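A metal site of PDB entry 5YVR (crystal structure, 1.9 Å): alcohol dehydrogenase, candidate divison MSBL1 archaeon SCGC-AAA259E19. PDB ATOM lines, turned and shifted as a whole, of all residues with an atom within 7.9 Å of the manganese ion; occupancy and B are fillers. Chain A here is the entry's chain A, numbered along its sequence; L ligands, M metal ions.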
ATOM      1  N   GLY A 160      25.532  22.145 -25.573  1.00  0.00           N
ATOM      2  CA  GLY A 160      24.586  22.741 -24.708  1.00  0.00           C
ATOM      3  C   GLY A 160      23.447  23.324 -25.482  1.00  0.00           C
ATOM      4  O   GLY A 160      22.353  22.802 -25.312  1.00  0.00           O
ATOM      5  N   THR A 161      23.639  24.410 -26.270  1.00  0.00           N
ATOM      6  CA  THR A 161      22.473  25.180 -26.678  1.00  0.00           C
ATOM      7  C   THR A 161      21.948  24.942 -28.118  1.00  0.00           C
ATOM      8  O   THR A 161      20.820  25.355 -28.424  1.00  0.00           O
ATOM      9  CB  THR A 161      22.728  26.700 -26.501  1.00  0.00           C
ATOM     10  OG1 THR A 161      23.609  27.135 -27.530  1.00  0.00           O
ATOM     11  CG2 THR A 161      23.257  27.035 -25.054  1.00  0.00           C
ATOM     12  N   GLY A 162      22.660  24.252 -28.993  1.00  0.00           N
ATOM     13  CA  GLY A 162      22.202  24.184 -30.386  1.00  0.00           C
ATOM     14  C   GLY A 162      22.318  25.510 -31.150  1.00  0.00           C
ATOM     15  O   GLY A 162      22.053  25.552 -32.381  1.00  0.00           O
ATOM     16  N   VAL A 170      18.711  34.747 -27.663  1.00  0.00           N
ATOM     17  CA  VAL A 170      17.958  34.921 -26.423  1.00  0.00           C
ATOM     18  C   VAL A 170      18.612  36.066 -25.653  1.00  0.00           C
ATOM     19  O   VAL A 170      19.733  35.918 -25.143  1.00  0.00           O
ATOM     20  CB  VAL A 170      17.894  33.623 -25.618  1.00  0.00           C
ATOM     21  CG1 VAL A 170      17.291  33.878 -24.197  1.00  0.00           C
ATOM     22  CG2 VAL A 170      17.059  32.545 -26.366  1.00  0.00           C
ATOM     23  N   ILE A 209      25.140  20.903 -17.119  1.00  0.00           N
ATOM     24  CA  ILE A 209      24.121  21.920 -17.347  1.00  0.00           C
ATOM     25  C   ILE A 209      23.793  22.001 -18.847  1.00  0.00           C
ATOM     26  O   ILE A 209      22.622  21.969 -19.261  1.00  0.00           O
ATOM     27  CB  ILE A 209      24.608  23.274 -16.807  1.00  0.00           C
ATOM     28  CG1 ILE A 209      24.858  23.201 -15.315  1.00  0.00           C
ATOM     29  CG2 ILE A 209      23.578  24.365 -17.033  1.00  0.00           C
ATOM     30  CD1 ILE A 209      23.568  23.382 -14.595  1.00  0.00           C
ATOM     31  N   THR A 210      24.818  22.111 -19.669  1.00  0.00           N
ATOM     32  CA  THR A 210      24.569  22.266 -21.102  1.00  0.00           C
ATOM     33  C   THR A 210      24.051  20.957 -21.692  1.00  0.00           C
ATOM     34  O   THR A 210      23.203  20.954 -22.596  1.00  0.00           O
ATOM     35  CB  THR A 210      25.840  22.726 -21.820  1.00  0.00           C
ATOM     36  OG1 THR A 210      26.851  21.707 -21.776  1.00  0.00           O
ATOM     37  CG2 THR A 210      26.364  24.039 -21.181  1.00  0.00           C
ATOM     38  N   TYR A 212      22.035  18.946 -20.122  1.00  0.00           N
ATOM     39  CA  TYR A 212      20.603  18.931 -19.830  1.00  0.00           C
ATOM     40  C   TYR A 212      19.828  19.850 -20.784  1.00  0.00           C
ATOM     41  O   TYR A 212      18.657  19.591 -21.083  1.00  0.00           O
ATOM     42  CB  TYR A 212      20.339  19.334 -18.359  1.00  0.00           C
ATOM     43  CG  TYR A 212      18.881  19.109 -18.033  1.00  0.00           C
ATOM     44  CD1 TYR A 212      18.386  17.818 -17.934  1.00  0.00           C
ATOM     45  CD2 TYR A 212      17.998  20.165 -17.938  1.00  0.00           C
ATOM     46  CE1 TYR A 212      17.044  17.584 -17.728  1.00  0.00           C
ATOM     47  CE2 TYR A 212      16.674  19.941 -17.710  1.00  0.00           C
ATOM     48  CZ  TYR A 212      16.189  18.638 -17.628  1.00  0.00           C
ATOM     49  OH  TYR A 212      14.837  18.400 -17.412  1.00  0.00           O
ATOM     50  N   ASP A 213      20.479  20.931 -21.250  1.00  0.00           N
ATOM     51  CA  ASP A 213      19.844  21.808 -22.232  1.00  0.00           C
ATOM     52  C   ASP A 213      19.530  21.063 -23.536  1.00  0.00           C
ATOM     53  O   ASP A 213      18.439  21.217 -24.087  1.00  0.00           O
ATOM     54  CB  ASP A 213      20.727  23.020 -22.510  1.00  0.00           C
ATOM     55  CG  ASP A 213      19.953  24.221 -23.068  1.00  0.00           C
ATOM     56  OD1 ASP A 213      18.723  24.216 -23.197  1.00  0.00           O
ATOM     57  OD2 ASP A 213      20.613  25.233 -23.371  1.00  0.00           O
ATOM     58  N   VAL A 214      20.492  20.258 -24.017  1.00  0.00           N
ATOM     59  CA  VAL A 214      20.280  19.394 -25.174  1.00  0.00           C
ATOM     60  C   VAL A 214      19.037  18.529 -24.972  1.00  0.00           C
ATOM     61  O   VAL A 214      18.166  18.419 -25.864  1.00  0.00           O
ATOM     62  CB  VAL A 214      21.518  18.505 -25.420  1.00  0.00           C
ATOM     63  CG1 VAL A 214      21.180  17.506 -26.603  1.00  0.00           C
ATOM     64  CG2 VAL A 214      22.733  19.367 -25.775  1.00  0.00           C
ATOM     65  N   SER A 216      16.633  18.999 -22.903  1.00  0.00           N
ATOM     66  CA  SER A 216      15.407  19.796 -22.749  1.00  0.00           C
ATOM     67  C   SER A 216      14.849  20.217 -24.100  1.00  0.00           C
ATOM     68  O   SER A 216      13.635  20.129 -24.343  1.00  0.00           O
ATOM     69  CB  SER A 216      15.625  21.033 -21.891  1.00  0.00           C
ATOM     70  OG  SER A 216      16.151  20.664 -20.619  1.00  0.00           O
ATOM     71  N   HIS A 217      15.732  20.658 -24.981  1.00  0.00           N
ATOM     72  CA  HIS A 217      15.291  21.045 -26.318  1.00  0.00           C
ATOM     73  C   HIS A 217      14.536  19.906 -27.007  1.00  0.00           C
ATOM     74  O   HIS A 217      13.420  20.090 -27.496  1.00  0.00           O
ATOM     75  CB  HIS A 217      16.494  21.450 -27.146  1.00  0.00           C
ATOM     76  CG  HIS A 217      17.055  22.783 -26.740  1.00  0.00           C
ATOM     77  ND1 HIS A 217      18.399  23.085 -26.812  1.00  0.00           N
ATOM     78  CD2 HIS A 217      16.458  23.884 -26.229  1.00  0.00           C
ATOM     79  CE1 HIS A 217      18.603  24.318 -26.381  1.00  0.00           C
ATOM     80  NE2 HIS A 217      17.439  24.827 -26.040  1.00  0.00           N
ATOM     81  N   GLU A 220      11.136  18.707 -25.559  1.00  0.00           N
ATOM     82  CA  GLU A 220      10.032  19.622 -25.863  1.00  0.00           C
ATOM     83  C   GLU A 220       9.745  19.645 -27.371  1.00  0.00           C
ATOM     84  O   GLU A 220       8.578  19.726 -27.770  1.00  0.00           O
ATOM     85  CB  GLU A 220      10.353  21.028 -25.345  1.00  0.00           C
ATOM     86  CG  GLU A 220      10.344  21.184 -23.741  1.00  0.00           C
ATOM     87  CD  GLU A 220      10.891  22.565 -23.318  1.00  0.00           C
ATOM     88  OE1 GLU A 220      12.011  22.567 -22.792  1.00  0.00           O
ATOM     89  OE2 GLU A 220      10.259  23.623 -23.640  1.00  0.00           O
ATOM     90  N   ASN A 273      15.163  22.018 -32.922  1.00  0.00           N
ATOM     91  CA  ASN A 273      14.511  23.196 -32.357  1.00  0.00           C
ATOM     92  C   ASN A 273      14.184  24.250 -33.429  1.00  0.00           C
ATOM     93  O   ASN A 273      13.197  24.992 -33.298  1.00  0.00           O
ATOM     94  CB  ASN A 273      15.393  23.770 -31.257  1.00  0.00           C
ATOM     95  CG  ASN A 273      14.662  24.745 -30.343  1.00  0.00           C
ATOM     96  OD1 ASN A 273      13.469  24.635 -30.083  1.00  0.00           O
ATOM     97  ND2 ASN A 273      15.395  25.723 -29.852  1.00  0.00           N
ATOM     98  N   THR A 278      10.150  24.915 -28.736  1.00  0.00           N
ATOM     99  CA  THR A 278      10.108  24.485 -27.335  1.00  0.00           C
ATOM    100  C   THR A 278       8.730  24.823 -26.751  1.00  0.00           C
ATOM    101  O   THR A 278       7.899  25.479 -27.373  1.00  0.00           O
ATOM    102  CB  THR A 278      11.268  25.103 -26.514  1.00  0.00           C
ATOM    103  OG1 THR A 278      11.304  26.526 -26.663  1.00  0.00           O
ATOM    104  CG2 THR A 278      12.610  24.537 -26.979  1.00  0.00           C
ATOM    105  N   ARG A 281       8.216  24.321 -20.568  1.00  0.00           N
ATOM    106  CA  ARG A 281       9.435  24.334 -19.758  1.00  0.00           C
ATOM    107  C   ARG A 281      10.328  25.517 -20.141  1.00  0.00           C
ATOM    108  O   ARG A 281      10.852  26.251 -19.270  1.00  0.00           O
ATOM    109  CB  ARG A 281      10.170  22.998 -19.893  1.00  0.00           C
ATOM    110  CG  ARG A 281      11.379  22.804 -18.939  1.00  0.00           C
ATOM    111  CD  ARG A 281      12.296  21.636 -19.412  1.00  0.00           C
ATOM    112  NE  ARG A 281      11.632  20.327 -19.411  1.00  0.00           N
ATOM    113  CZ  ARG A 281      11.729  19.411 -20.388  1.00  0.00           C
ATOM    114  NH1 ARG A 281      12.445  19.675 -21.477  1.00  0.00           N
ATOM    115  NH2 ARG A 281      11.073  18.228 -20.313  1.00  0.00           N
ATOM    116  N   HIS A 282      10.512  25.751 -21.434  1.00  0.00           N
ATOM    117  CA  HIS A 282      11.323  26.891 -21.853  1.00  0.00           C
ATOM    118  C   HIS A 282      10.635  28.209 -21.557  1.00  0.00           C
ATOM    119  O   HIS A 282      11.279  29.172 -21.137  1.00  0.00           O
ATOM    120  CB  HIS A 282      11.692  26.802 -23.320  1.00  0.00           C
ATOM    121  CG  HIS A 282      13.001  26.148 -23.525  1.00  0.00           C
ATOM    122  ND1 HIS A 282      13.197  24.804 -23.275  1.00  0.00           N
ATOM    123  CD2 HIS A 282      14.215  26.671 -23.796  1.00  0.00           C
ATOM    124  CE1 HIS A 282      14.480  24.511 -23.456  1.00  0.00           C
ATOM    125  NE2 HIS A 282      15.101  25.629 -23.789  1.00  0.00           N
ATOM    126  N   ALA A 285      11.323  28.836 -17.893  1.00  0.00           N
ATOM    127  CA  ALA A 285      12.718  28.997 -17.476  1.00  0.00           C
ATOM    128  C   ALA A 285      13.273  30.356 -17.877  1.00  0.00           C
ATOM    129  O   ALA A 285      14.199  30.867 -17.225  1.00  0.00           O
ATOM    130  CB  ALA A 285      13.574  27.873 -18.069  1.00  0.00           C
ATOM    131  N   HIS A 297      20.658  28.893 -17.425  1.00  0.00           N
ATOM    132  CA  HIS A 297      19.499  28.444 -18.199  1.00  0.00           C
ATOM    133  C   HIS A 297      19.151  26.978 -17.936  1.00  0.00           C
ATOM    134  O   HIS A 297      17.996  26.659 -17.641  1.00  0.00           O
ATOM    135  CB  HIS A 297      19.816  28.653 -19.674  1.00  0.00           C
ATOM    136  CG  HIS A 297      18.730  28.220 -20.598  1.00  0.00           C
ATOM    137  ND1 HIS A 297      17.431  28.679 -20.480  1.00  0.00           N
ATOM    138  CD2 HIS A 297      18.742  27.362 -21.640  1.00  0.00           C
ATOM    139  CE1 HIS A 297      16.693  28.119 -21.416  1.00  0.00           C
ATOM    140  NE2 HIS A 297      17.469  27.354 -22.160  1.00  0.00           N
ATOM    141  N   GLY A 298      20.110  26.069 -18.119  1.00  0.00           N
ATOM    142  CA  GLY A 298      19.836  24.654 -17.927  1.00  0.00           C
ATOM    143  C   GLY A 298      19.485  24.253 -16.489  1.00  0.00           C
ATOM    144  O   GLY A 298      18.668  23.318 -16.281  1.00  0.00           O
ATOM    145  N   LEU A 301      15.899  25.219 -16.261  1.00  0.00           N
ATOM    146  CA  LEU A 301      15.081  24.185 -16.890  1.00  0.00           C
ATOM    147  C   LEU A 301      14.940  22.979 -15.953  1.00  0.00           C
ATOM    148  O   LEU A 301      13.830  22.467 -15.732  1.00  0.00           O
ATOM    149  CB  LEU A 301      15.690  23.738 -18.217  1.00  0.00           C
ATOM    150  CG  LEU A 301      15.847  24.830 -19.282  1.00  0.00           C
ATOM    151  CD1 LEU A 301      16.696  24.366 -20.428  1.00  0.00           C
ATOM    152  CD2 LEU A 301      14.464  25.123 -19.803  1.00  0.00           C
HETATM  153  P1  LIG L   1      27.293  30.414 -21.704  1.00  0.00           P
HETATM  154  O1  LIG L   1      27.611  30.735 -23.148  1.00  0.00           O
HETATM  155  O2  LIG L   1      26.196  31.281 -21.138  1.00  0.00           O
HETATM  156  O3  LIG L   1      28.543  30.644 -20.797  1.00  0.00           O
HETATM  157  C1  LIG L   1      29.102  29.500 -20.541  1.00  0.00           C
HETATM  158  C2  LIG L   1      30.045  29.679 -19.355  1.00  0.00           C
HETATM  159  O4  LIG L   1      30.927  28.655 -19.436  1.00  0.00           O
HETATM  160  C3  LIG L   1      30.928  31.063 -19.462  1.00  0.00           C
HETATM  161  O5  LIG L   1      31.432  31.466 -18.203  1.00  0.00           O
HETATM  162  C4  LIG L   1      32.117  30.604 -20.343  1.00  0.00           C
HETATM  163  O6  LIG L   1      33.320  31.224 -20.138  1.00  0.00           O
HETATM  164  C5  LIG L   1      32.265  29.165 -19.872  1.00  0.00           C
HETATM  165  N1  LIG L   1      32.641  28.331 -20.926  1.00  0.00           N
HETATM  166  C6  LIG L   1      32.002  28.185 -22.188  1.00  0.00           C
HETATM  167  N2  LIG L   1      32.576  27.246 -22.947  1.00  0.00           N
HETATM  168  C7  LIG L   1      33.577  26.738 -22.147  1.00  0.00           C
HETATM  169  C8  LIG L   1      34.528  25.745 -22.354  1.00  0.00           C
HETATM  170  N3  LIG L   1      34.580  25.054 -23.520  1.00  0.00           N
HETATM  171  N4  LIG L   1      35.438  25.433 -21.388  1.00  0.00           N
HETATM  172  C9  LIG L   1      35.337  26.186 -20.252  1.00  0.00           C
HETATM  173  N5  LIG L   1      34.523  27.164 -19.931  1.00  0.00           N
HETATM  174  C10 LIG L   1      33.631  27.429 -20.891  1.00  0.00           C
HETATM  175  O7  LIG L   1      26.863  28.759 -21.605  1.00  0.00           O
HETATM  176  P2  LIG L   1      25.629  28.283 -22.566  1.00  0.00           P
HETATM  177  O8  LIG L   1      26.220  28.032 -23.883  1.00  0.00           O
HETATM  178  O9  LIG L   1      24.804  27.257 -21.800  1.00  0.00           O
HETATM  179  O10 LIG L   1      24.627  29.663 -22.573  1.00  0.00           O
HETATM  180  C11 LIG L   1      23.679  29.499 -23.182  1.00  0.00           C
HETATM  181  C12 LIG L   1      22.890  30.759 -23.368  1.00  0.00           C
HETATM  182  O11 LIG L   1      22.192  30.319 -24.449  1.00  0.00           O
HETATM  183  C13 LIG L   1      21.792  31.181 -22.325  1.00  0.00           C
HETATM  184  O12 LIG L   1      21.674  32.602 -22.344  1.00  0.00           O
HETATM  185  C14 LIG L   1      20.497  30.638 -22.902  1.00  0.00           C
HETATM  186  O13 LIG L   1      19.358  31.425 -22.720  1.00  0.00           O
HETATM  187  C15 LIG L   1      20.839  30.708 -24.404  1.00  0.00           C
HETATM  188  N6  LIG L   1      20.137  29.710 -25.256  1.00  0.00           N
HETATM  189  C16 LIG L   1      19.946  30.009 -26.569  1.00  0.00           C
HETATM  190  C17 LIG L   1      19.387  29.130 -27.457  1.00  0.00           C
HETATM  191  C18 LIG L   1      19.257  29.582 -28.889  1.00  0.00           C
HETATM  192  O14 LIG L   1      19.584  30.715 -29.342  1.00  0.00           O
HETATM  193  N7  LIG L   1      18.714  28.623 -29.809  1.00  0.00           N
HETATM  194  C19 LIG L   1      18.969  27.729 -27.027  1.00  0.00           C
HETATM  195  C20 LIG L   1      19.173  27.459 -25.504  1.00  0.00           C
HETATM  196  C21 LIG L   1      19.702  28.392 -24.712  1.00  0.00           C
HETATM  197  P3  LIG L   1      33.327  32.935 -20.503  1.00  0.00           P
HETATM  198  O15 LIG L   1      32.600  32.964 -21.811  1.00  0.00           O
HETATM  199  O16 LIG L   1      32.601  33.627 -19.354  1.00  0.00           O
HETATM  200  O17 LIG L   1      34.825  33.102 -20.560  1.00  0.00           O
HETATM  201 MN    MN M   1      17.374  25.729 -23.732  1.00  0.00          MN
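The side-chain carboxylate (OE1) of Glu 220 lies within hydrogen-bond range of a ring nitrogen (ND1) of His 282.
CD1 of Leu 301 touches the manganese ion, 3.6 Å away. The nearest printed residue that does not touch the manganese ion is Ser 216 (5.3 Å).
The manganese ion is bound by the side-chain carboxylate (OD1) of Asp 213 (2.1 Å), a ring nitrogen (NE2) of His 297 (2.3 Å), a ring nitrogen (NE2) of His 282 (2.3 Å) and a ring nitrogen (NE2) of His 217 (2.5 Å). The manganese ion has four donor atoms within binding distance.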
